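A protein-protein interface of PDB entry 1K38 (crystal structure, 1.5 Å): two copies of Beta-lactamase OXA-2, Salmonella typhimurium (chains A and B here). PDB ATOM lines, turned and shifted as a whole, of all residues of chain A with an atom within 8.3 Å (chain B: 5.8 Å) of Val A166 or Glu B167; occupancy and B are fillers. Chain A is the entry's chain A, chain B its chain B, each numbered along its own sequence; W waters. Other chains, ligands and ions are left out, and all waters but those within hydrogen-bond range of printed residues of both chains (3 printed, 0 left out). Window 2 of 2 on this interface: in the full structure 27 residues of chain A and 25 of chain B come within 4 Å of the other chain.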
ATOM      1  N   LEU A  59      13.690  -8.399   8.218  1.00  0.00           N
ATOM      2  CA  LEU A  59      13.519  -7.505   9.360  1.00  0.00           C
ATOM      3  C   LEU A  59      14.852  -7.424  10.109  1.00  0.00           C
ATOM      4  O   LEU A  59      15.290  -6.338  10.487  1.00  0.00           O
ATOM      5  CB  LEU A  59      12.423  -8.020  10.299  1.00  0.00           C
ATOM      6  CG  LEU A  59      10.991  -8.049   9.754  1.00  0.00           C
ATOM      7  CD1 LEU A  59      10.084  -8.769  10.741  1.00  0.00           C
ATOM      8  CD2 LEU A  59      10.504  -6.623   9.517  1.00  0.00           C
ATOM      9  N   LEU A  62      17.292  -5.244   8.059  1.00  0.00           N
ATOM     10  CA  LEU A  62      16.963  -3.823   8.065  1.00  0.00           C
ATOM     11  C   LEU A  62      17.292  -3.229   9.434  1.00  0.00           C
ATOM     12  O   LEU A  62      17.835  -2.125   9.533  1.00  0.00           O
ATOM     13  CB  LEU A  62      15.475  -3.622   7.759  1.00  0.00           C
ATOM     14  CG  LEU A  62      15.040  -3.858   6.308  1.00  0.00           C
ATOM     15  CD1 LEU A  62      13.535  -4.092   6.266  1.00  0.00           C
ATOM     16  CD2 LEU A  62      15.433  -2.666   5.444  1.00  0.00           C
ATOM     17  N   LEU A 157       3.151  -9.929  12.376  1.00  0.00           N
ATOM     18  CA  LEU A 157       3.656  -9.038  11.333  1.00  0.00           C
ATOM     19  C   LEU A 157       2.504  -8.206  10.764  1.00  0.00           C
ATOM     20  O   LEU A 157       2.621  -6.996  10.570  1.00  0.00           O
ATOM     21  CB  LEU A 157       4.303  -9.858  10.206  1.00  0.00           C
ATOM     22  CG  LEU A 157       4.791  -9.073   8.982  1.00  0.00           C
ATOM     23  CD1 LEU A 157       5.828  -8.036   9.405  1.00  0.00           C
ATOM     24  CD2 LEU A 157       5.394 -10.036   7.957  1.00  0.00           C
ATOM     25  N   ARG A 159      -0.226  -7.326  12.155  1.00  0.00           N
ATOM     26  CA  ARG A 159      -0.662  -6.345  13.144  1.00  0.00           C
ATOM     27  C   ARG A 159       0.413  -5.336  13.540  1.00  0.00           C
ATOM     28  O   ARG A 159       0.163  -4.472  14.383  1.00  0.00           O
ATOM     29  CB  ARG A 159      -1.157  -7.070  14.400  1.00  0.00           C
ATOM     30  CG  ARG A 159      -2.351  -7.984  14.176  1.00  0.00           C
ATOM     31  CD  ARG A 159      -3.628  -7.180  13.993  1.00  0.00           C
ATOM     32  NE  ARG A 159      -4.769  -8.034  13.682  1.00  0.00           N
ATOM     33  CZ  ARG A 159      -6.012  -7.591  13.526  1.00  0.00           C
ATOM     34  NH1 ARG A 159      -6.279  -6.299  13.659  1.00  0.00           N
ATOM     35  NH2 ARG A 159      -6.987  -8.439  13.222  1.00  0.00           N
ATOM     36  N   ASN A 160       1.596  -5.442  12.937  1.00  0.00           N
ATOM     37  CA  ASN A 160       2.710  -4.541  13.245  1.00  0.00           C
ATOM     38  C   ASN A 160       3.145  -4.727  14.696  1.00  0.00           C
ATOM     39  O   ASN A 160       3.668  -3.802  15.318  1.00  0.00           O
ATOM     40  CB  ASN A 160       2.296  -3.082  13.017  1.00  0.00           C
ATOM     41  CG  ASN A 160       1.830  -2.823  11.596  1.00  0.00           C
ATOM     42  OD1 ASN A 160       2.558  -3.083  10.635  1.00  0.00           O
ATOM     43  ND2 ASN A 160       0.609  -2.307  11.455  1.00  0.00           N
ATOM     44  N   GLU A 161       2.953  -5.937  15.216  1.00  0.00           N
ATOM     45  CA  GLU A 161       3.283  -6.259  16.605  1.00  0.00           C
ATOM     46  C   GLU A 161       4.682  -6.807  16.860  1.00  0.00           C
ATOM     47  O   GLU A 161       5.035  -7.081  18.008  1.00  0.00           O
ATOM     48  CB  GLU A 161       2.274  -7.263  17.161  1.00  0.00           C
ATOM     49  CG  GLU A 161       0.834  -6.827  17.063  1.00  0.00           C
ATOM     50  CD  GLU A 161      -0.117  -7.894  17.561  1.00  0.00           C
ATOM     51  OE1 GLU A 161       0.171  -9.093  17.352  1.00  0.00           O
ATOM     52  OE2 GLU A 161      -1.153  -7.538  18.151  1.00  0.00           O
ATOM     53  N   LEU A 162       5.477  -6.987  15.811  1.00  0.00           N
ATOM     54  CA  LEU A 162       6.825  -7.503  16.013  1.00  0.00           C
ATOM     55  C   LEU A 162       7.709  -6.392  16.576  1.00  0.00           C
ATOM     56  O   LEU A 162       7.458  -5.206  16.345  1.00  0.00           O
ATOM     57  CB  LEU A 162       7.397  -8.034  14.699  1.00  0.00           C
ATOM     58  CG  LEU A 162       6.680  -9.259  14.116  1.00  0.00           C
ATOM     59  CD1 LEU A 162       7.265  -9.574  12.749  1.00  0.00           C
ATOM     60  CD2 LEU A 162       6.821 -10.463  15.051  1.00  0.00           C
ATOM     61  N   PRO A 163       8.754  -6.762  17.332  1.00  0.00           N
ATOM     62  CA  PRO A 163       9.679  -5.797  17.935  1.00  0.00           C
ATOM     63  C   PRO A 163      10.693  -5.212  16.955  1.00  0.00           C
ATOM     64  O   PRO A 163      11.906  -5.293  17.167  1.00  0.00           O
ATOM     65  CB  PRO A 163      10.344  -6.612  19.035  1.00  0.00           C
ATOM     66  CG  PRO A 163      10.456  -7.958  18.396  1.00  0.00           C
ATOM     67  CD  PRO A 163       9.093  -8.138  17.743  1.00  0.00           C
ATOM     68  N   PHE A 164      10.178  -4.618  15.882  1.00  0.00           N
ATOM     69  CA  PHE A 164      10.997  -3.987  14.853  1.00  0.00           C
ATOM     70  C   PHE A 164      10.290  -2.701  14.454  1.00  0.00           C
ATOM     71  O   PHE A 164       9.096  -2.550  14.703  1.00  0.00           O
ATOM     72  CB  PHE A 164      11.108  -4.892  13.621  1.00  0.00           C
ATOM     73  CG  PHE A 164      11.888  -6.149  13.860  1.00  0.00           C
ATOM     74  CD1 PHE A 164      13.278  -6.135  13.845  1.00  0.00           C
ATOM     75  CD2 PHE A 164      11.233  -7.345  14.131  1.00  0.00           C
ATOM     76  CE1 PHE A 164      14.004  -7.296  14.100  1.00  0.00           C
ATOM     77  CE2 PHE A 164      11.950  -8.508  14.387  1.00  0.00           C
ATOM     78  CZ  PHE A 164      13.338  -8.483  14.372  1.00  0.00           C
ATOM     79  N   ARG A 165      11.025  -1.776  13.846  1.00  0.00           N
ATOM     80  CA  ARG A 165      10.433  -0.519  13.395  1.00  0.00           C
ATOM     81  C   ARG A 165       9.223  -0.840  12.531  1.00  0.00           C
ATOM     82  O   ARG A 165       9.287  -1.732  11.682  1.00  0.00           O
ATOM     83  CB  ARG A 165      11.425   0.279  12.543  1.00  0.00           C
ATOM     84  CG  ARG A 165      12.661   0.772  13.268  1.00  0.00           C
ATOM     85  CD  ARG A 165      13.600   1.459  12.286  1.00  0.00           C
ATOM     86  NE  ARG A 165      14.818   1.949  12.925  1.00  0.00           N
ATOM     87  CZ  ARG A 165      15.148   3.233  13.024  1.00  0.00           C
ATOM     88  NH1 ARG A 165      14.348   4.167  12.525  1.00  0.00           N
ATOM     89  NH2 ARG A 165      16.279   3.583  13.626  1.00  0.00           N
ATOM     90  N   VAL A 166       8.130  -0.115  12.732  1.00  0.00           N
ATOM     91  CA  VAL A 166       6.944  -0.354  11.924  1.00  0.00           C
ATOM     92  C   VAL A 166       7.278  -0.139  10.444  1.00  0.00           C
ATOM     93  O   VAL A 166       6.741  -0.834   9.576  1.00  0.00           O
ATOM     94  CB  VAL A 166       5.776   0.559  12.358  1.00  0.00           C
ATOM     95  CG1 VAL A 166       4.647   0.515  11.325  1.00  0.00           C
ATOM     96  CG2 VAL A 166       5.257   0.099  13.714  1.00  0.00           C
ATOM     97  N   GLU A 167       8.173   0.804  10.144  1.00  0.00           N
ATOM     98  CA  GLU A 167       8.536   1.033   8.748  1.00  0.00           C
ATOM     99  C   GLU A 167       9.126  -0.239   8.133  1.00  0.00           C
ATOM    100  O   GLU A 167       8.873  -0.541   6.958  1.00  0.00           O
ATOM    101  CB  GLU A 167       9.534   2.198   8.609  1.00  0.00           C
ATOM    102  CG  GLU A 167      10.863   2.024   9.325  1.00  0.00           C
ATOM    103  CD  GLU A 167      11.899   3.039   8.868  1.00  0.00           C
ATOM    104  OE1 GLU A 167      12.179   3.093   7.651  1.00  0.00           O
ATOM    105  OE2 GLU A 167      12.440   3.779   9.723  1.00  0.00           O
ATOM    106  N   HIS A 168       9.894  -0.989   8.926  1.00  0.00           N
ATOM    107  CA  HIS A 168      10.504  -2.222   8.427  1.00  0.00           C
ATOM    108  C   HIS A 168       9.455  -3.310   8.245  1.00  0.00           C
ATOM    109  O   HIS A 168       9.511  -4.083   7.282  1.00  0.00           O
ATOM    110  CB  HIS A 168      11.596  -2.710   9.381  1.00  0.00           C
ATOM    111  CG  HIS A 168      12.798  -1.821   9.422  1.00  0.00           C
ATOM    112  ND1 HIS A 168      13.087  -0.913   8.425  1.00  0.00           N
ATOM    113  CD2 HIS A 168      13.799  -1.718  10.328  1.00  0.00           C
ATOM    114  CE1 HIS A 168      14.216  -0.290   8.716  1.00  0.00           C
ATOM    115  NE2 HIS A 168      14.667  -0.760   9.864  1.00  0.00           N
ATOM    116  N   GLN A 169       8.502  -3.375   9.166  1.00  0.00           N
ATOM    117  CA  GLN A 169       7.433  -4.362   9.058  1.00  0.00           C
ATOM    118  C   GLN A 169       6.592  -4.059   7.821  1.00  0.00           C
ATOM    119  O   GLN A 169       6.186  -4.977   7.101  1.00  0.00           O
ATOM    120  CB  GLN A 169       6.565  -4.359  10.321  1.00  0.00           C
ATOM    121  CG  GLN A 169       7.324  -4.778  11.575  1.00  0.00           C
ATOM    122  CD  GLN A 169       6.434  -4.850  12.802  1.00  0.00           C
ATOM    123  OE1 GLN A 169       5.609  -5.755  12.936  1.00  0.00           O
ATOM    124  NE2 GLN A 169       6.594  -3.888  13.706  1.00  0.00           N
ATOM    125  N   ARG A 170       6.340  -2.780   7.555  1.00  0.00           N
ATOM    126  CA  ARG A 170       5.562  -2.420   6.375  1.00  0.00           C
ATOM    127  C   ARG A 170       6.324  -2.736   5.090  1.00  0.00           C
ATOM    128  O   ARG A 170       5.742  -3.227   4.121  1.00  0.00           O
ATOM    129  CB  ARG A 170       5.181  -0.940   6.402  1.00  0.00           C
ATOM    130  CG  ARG A 170       4.231  -0.590   7.528  1.00  0.00           C
ATOM    131  CD  ARG A 170       3.549   0.756   7.301  1.00  0.00           C
ATOM    132  NE  ARG A 170       2.708   1.104   8.444  1.00  0.00           N
ATOM    133  CZ  ARG A 170       1.584   0.478   8.777  1.00  0.00           C
ATOM    134  NH1 ARG A 170       1.129  -0.537   8.045  1.00  0.00           N
ATOM    135  NH2 ARG A 170       0.935   0.835   9.879  1.00  0.00           N
ATOM    136  N   LEU A 171       7.626  -2.462   5.074  1.00  0.00           N
ATOM    137  CA  LEU A 171       8.421  -2.759   3.892  1.00  0.00           C
ATOM    138  C   LEU A 171       8.396  -4.257   3.603  1.00  0.00           C
ATOM    139  O   LEU A 171       8.232  -4.667   2.451  1.00  0.00           O
ATOM    140  CB  LEU A 171       9.870  -2.290   4.073  1.00  0.00           C
ATOM    141  CG  LEU A 171      10.833  -2.654   2.935  1.00  0.00           C
ATOM    142  CD1 LEU A 171      10.247  -2.217   1.594  1.00  0.00           C
ATOM    143  CD2 LEU A 171      12.194  -1.990   3.177  1.00  0.00           C
ATOM    144  N   VAL A 172       8.554  -5.083   4.633  1.00  0.00           N
ATOM    145  CA  VAL A 172       8.538  -6.522   4.411  1.00  0.00           C
ATOM    146  C   VAL A 172       7.176  -6.980   3.885  1.00  0.00           C
ATOM    147  O   VAL A 172       7.113  -7.805   2.979  1.00  0.00           O
ATOM    148  CB  VAL A 172       8.904  -7.296   5.701  1.00  0.00           C
ATOM    149  CG1 VAL A 172       8.676  -8.794   5.500  1.00  0.00           C
ATOM    150  CG2 VAL A 172      10.364  -7.050   6.046  1.00  0.00           C
ATOM    151  N   LYS A 173       6.086  -6.447   4.435  1.00  0.00           N
ATOM    152  CA  LYS A 173       4.763  -6.846   3.953  1.00  0.00           C
ATOM    153  C   LYS A 173       4.565  -6.422   2.503  1.00  0.00           C
ATOM    154  O   LYS A 173       3.845  -7.076   1.746  1.00  0.00           O
ATOM    155  CB  LYS A 173       3.659  -6.274   4.854  1.00  0.00           C
ATOM    156  CG  LYS A 173       3.546  -7.031   6.171  1.00  0.00           C
ATOM    157  CD  LYS A 173       2.413  -6.522   7.058  1.00  0.00           C
ATOM    158  CE  LYS A 173       2.755  -5.188   7.703  1.00  0.00           C
ATOM    159  NZ  LYS A 173       1.700  -4.742   8.660  1.00  0.00           N
ATOM    160  N   PHE B 164       7.678  13.174   5.831  1.00  0.00           N
ATOM    161  CA  PHE B 164       6.806  12.426   6.735  1.00  0.00           C
ATOM    162  C   PHE B 164       7.494  11.122   7.119  1.00  0.00           C
ATOM    163  O   PHE B 164       8.449  10.702   6.461  1.00  0.00           O
ATOM    164  CB  PHE B 164       5.471  12.115   6.048  1.00  0.00           C
ATOM    165  CG  PHE B 164       4.657  13.335   5.745  1.00  0.00           C
ATOM    166  CD1 PHE B 164       3.894  13.937   6.738  1.00  0.00           C
ATOM    167  CD2 PHE B 164       4.692  13.910   4.478  1.00  0.00           C
ATOM    168  CE1 PHE B 164       3.179  15.102   6.477  1.00  0.00           C
ATOM    169  CE2 PHE B 164       3.978  15.077   4.206  1.00  0.00           C
ATOM    170  CZ  PHE B 164       3.221  15.674   5.208  1.00  0.00           C
ATOM    171  N   ARG B 165       7.016  10.483   8.183  1.00  0.00           N
ATOM    172  CA  ARG B 165       7.614   9.226   8.614  1.00  0.00           C
ATOM    173  C   ARG B 165       7.657   8.268   7.443  1.00  0.00           C
ATOM    174  O   ARG B 165       6.713   8.196   6.660  1.00  0.00           O
ATOM    175  CB  ARG B 165       6.793   8.562   9.719  1.00  0.00           C
ATOM    176  CG  ARG B 165       6.640   9.361  10.989  1.00  0.00           C
ATOM    177  CD  ARG B 165       6.127   8.468  12.106  1.00  0.00           C
ATOM    178  NE  ARG B 165       7.172   7.574  12.599  1.00  0.00           N
ATOM    179  CZ  ARG B 165       7.059   6.826  13.694  1.00  0.00           C
ATOM    180  NH1 ARG B 165       5.942   6.854  14.409  1.00  0.00           N
ATOM    181  NH2 ARG B 165       8.083   6.084  14.102  1.00  0.00           N
ATOM    182  N   VAL B 166       8.745   7.524   7.325  1.00  0.00           N
ATOM    183  CA  VAL B 166       8.836   6.560   6.248  1.00  0.00           C
ATOM    184  C   VAL B 166       7.711   5.537   6.431  1.00  0.00           C
ATOM    185  O   VAL B 166       7.103   5.103   5.451  1.00  0.00           O
ATOM    186  CB  VAL B 166      10.211   5.853   6.232  1.00  0.00           C
ATOM    187  CG1 VAL B 166      10.185   4.688   5.253  1.00  0.00           C
ATOM    188  CG2 VAL B 166      11.295   6.851   5.826  1.00  0.00           C
ATOM    189  N   GLU B 167       7.403   5.160   7.674  1.00  0.00           N
ATOM    190  CA  GLU B 167       6.326   4.191   7.863  1.00  0.00           C
ATOM    191  C   GLU B 167       5.002   4.714   7.316  1.00  0.00           C
ATOM    192  O   GLU B 167       4.194   3.942   6.795  1.00  0.00           O
ATOM    193  CB  GLU B 167       6.160   3.786   9.336  1.00  0.00           C
ATOM    194  CG  GLU B 167       5.891   4.904  10.332  1.00  0.00           C
ATOM    195  CD  GLU B 167       5.477   4.357  11.688  1.00  0.00           C
ATOM    196  OE1 GLU B 167       4.257   4.215  11.935  1.00  0.00           O
ATOM    197  OE2 GLU B 167       6.373   4.044  12.503  1.00  0.00           O
ATOM    198  N   HIS B 168       4.779   6.021   7.416  1.00  0.00           N
ATOM    199  CA  HIS B 168       3.542   6.602   6.907  1.00  0.00           C
ATOM    200  C   HIS B 168       3.551   6.601   5.382  1.00  0.00           C
ATOM    201  O   HIS B 168       2.525   6.350   4.747  1.00  0.00           O
ATOM    202  CB  HIS B 168       3.352   8.030   7.420  1.00  0.00           C
ATOM    203  CG  HIS B 168       3.083   8.113   8.890  1.00  0.00           C
ATOM    204  ND1 HIS B 168       2.610   7.048   9.629  1.00  0.00           N
ATOM    205  CD2 HIS B 168       3.188   9.151   9.754  1.00  0.00           C
ATOM    206  CE1 HIS B 168       2.435   7.428  10.883  1.00  0.00           C
ATOM    207  NE2 HIS B 168       2.778   8.700  10.984  1.00  0.00           N
ATOM    208  N   GLN B 169       4.708   6.889   4.792  1.00  0.00           N
ATOM    209  CA  GLN B 169       4.821   6.875   3.337  1.00  0.00           C
ATOM    210  C   GLN B 169       4.601   5.446   2.837  1.00  0.00           C
ATOM    211  O   GLN B 169       3.941   5.237   1.816  1.00  0.00           O
ATOM    212  CB  GLN B 169       6.188   7.406   2.893  1.00  0.00           C
ATOM    213  CG  GLN B 169       6.392   8.889   3.224  1.00  0.00           C
ATOM    214  CD  GLN B 169       7.721   9.426   2.728  1.00  0.00           C
ATOM    215  OE1 GLN B 169       7.928   9.591   1.525  1.00  0.00           O
ATOM    216  NE2 GLN B 169       8.635   9.692   3.658  1.00  0.00           N
ATOM    217  N   ARG B 170       5.130   4.459   3.557  1.00  0.00           N
ATOM    218  CA  ARG B 170       4.930   3.076   3.141  1.00  0.00           C
ATOM    219  C   ARG B 170       3.468   2.667   3.277  1.00  0.00           C
ATOM    220  O   ARG B 170       2.935   1.960   2.414  1.00  0.00           O
ATOM    221  CB  ARG B 170       5.821   2.129   3.952  1.00  0.00           C
ATOM    222  CG  ARG B 170       7.301   2.300   3.624  1.00  0.00           C
ATOM    223  CD  ARG B 170       8.156   1.200   4.226  1.00  0.00           C
ATOM    224  NE  ARG B 170       9.578   1.476   4.030  1.00  0.00           N
ATOM    225  CZ  ARG B 170      10.175   1.542   2.845  1.00  0.00           C
ATOM    226  NH1 ARG B 170       9.478   1.339   1.731  1.00  0.00           N
ATOM    227  NH2 ARG B 170      11.466   1.848   2.764  1.00  0.00           N
ATOM    228  N   LEU B 171       2.811   3.111   4.345  1.00  0.00           N
ATOM    229  CA  LEU B 171       1.406   2.770   4.531  1.00  0.00           C
ATOM    230  C   LEU B 171       0.559   3.348   3.393  1.00  0.00           C
ATOM    231  O   LEU B 171      -0.284   2.653   2.830  1.00  0.00           O
ATOM    232  CB  LEU B 171       0.896   3.285   5.885  1.00  0.00           C
ATOM    233  CG  LEU B 171      -0.602   3.108   6.163  1.00  0.00           C
ATOM    234  CD1 LEU B 171      -1.024   1.659   5.947  1.00  0.00           C
ATOM    235  CD2 LEU B 171      -0.896   3.541   7.593  1.00  0.00           C
ATOM    236  N   VAL B 172       0.788   4.609   3.041  1.00  0.00           N
ATOM    237  CA  VAL B 172       0.026   5.230   1.962  1.00  0.00           C
ATOM    238  C   VAL B 172       0.254   4.503   0.641  1.00  0.00           C
ATOM    239  O   VAL B 172      -0.693   4.294  -0.122  1.00  0.00           O
ATOM    240  CB  VAL B 172       0.385   6.729   1.821  1.00  0.00           C
ATOM    241  CG1 VAL B 172      -0.283   7.337   0.589  1.00  0.00           C
ATOM    242  CG2 VAL B 172      -0.071   7.472   3.072  1.00  0.00           C
HETATM  243  O   HOH W   1       2.604   3.601   9.891  1.00  0.00           O
HETATM  244  O   HOH W   2       8.759   3.197  11.778  1.00  0.00           O
HETATM  245  O   HOH W   3      11.725   1.182   5.977  1.00  0.00           O
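The guanidinium group (NH1) of Arg A165 lies within salt-bridge range of the side-chain carboxylate (OE2) of Glu A167. NH2 of Arg B165 is in salt-bridge range of OE2 of Glu B167.
Among the printed residues, merely in contact across the chains: Val A166 with Glu B167 (3.5 Å), Glu A167 with Val B166 (3.5 Å), Glu A167 with Glu B167 (3.7 Å), Glu A167 with Arg B170 (3.3 Å), Arg A170 with Glu B167 (3.3 Å), Arg A170 with Arg B170 (3.98 Å), Arg A170 with Leu B171 (3.7 Å) and Leu A171 with Arg B170 (3.6 Å).
Of chain B, only Glu B167 comes within 4 Å of Val A166. Glu B167 touches three residues of chain A. Of the printed residues of chain B, Glu A167 touches Val B166 (3.5 Å), Glu B167 (3.7 Å) and Arg B170 (3.3 Å). Printed residues of chain B within 4 Å of Leu A171: Arg B170 (3.6 Å). The nearest residue of chain A that does not touch Glu B167 is Arg A165 (5.7 Å). The nearest printed residue of chain A that does not touch Arg B170 is His A168 (5.5 Å).
Hydrophobic or aromatic side chains of chain B that line the printed part of chain A: Val B166 and Leu B171. Hydrophobic or aromatic side chains of chain A that line the printed part of chain B: Val A166 and Leu A171. Among the printed residues, no Asp or Glu carboxylate lies within 4 Å of a Lys or Arg side-chain nitrogen of the other chain.
Val A166 touches Glu B167, and with the chains exchanged Glu A167 touches Val B166. Glu A167 touches Arg B170, and with the chains exchanged Arg A170 touches Glu B167. Arg B170 touches its own counterpart, Arg A170. Arg A170 touches Leu B171, and with the chains exchanged Leu A171 touches Arg B170. Positions printed for both chains: 164, 165, 166, 167, 168, 169, 170, 171 and 172. Of the 8 pairs that touch across the chains among the printed residues, 8 have their exchanged pair printed and touching as well.
Water W3 lies within hydrogen-bond range of the side-chain carboxylate (OE1) of Glu A167, the guanidinium group (NE) of Arg B170 and a ring nitrogen (ND1) of His A168. Water W2 lies within hydrogen-bond range of the side-chain carboxylate of Glu B167 (2.6 Å) and the backbone NH of Glu A167 (3.0 Å). Water W1 lies within hydrogen-bond range of OE1 of Glu B167 (2.7 Å), NE of Arg A170 (2.9 Å) and ND1 of His B168 (3.5 Å).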
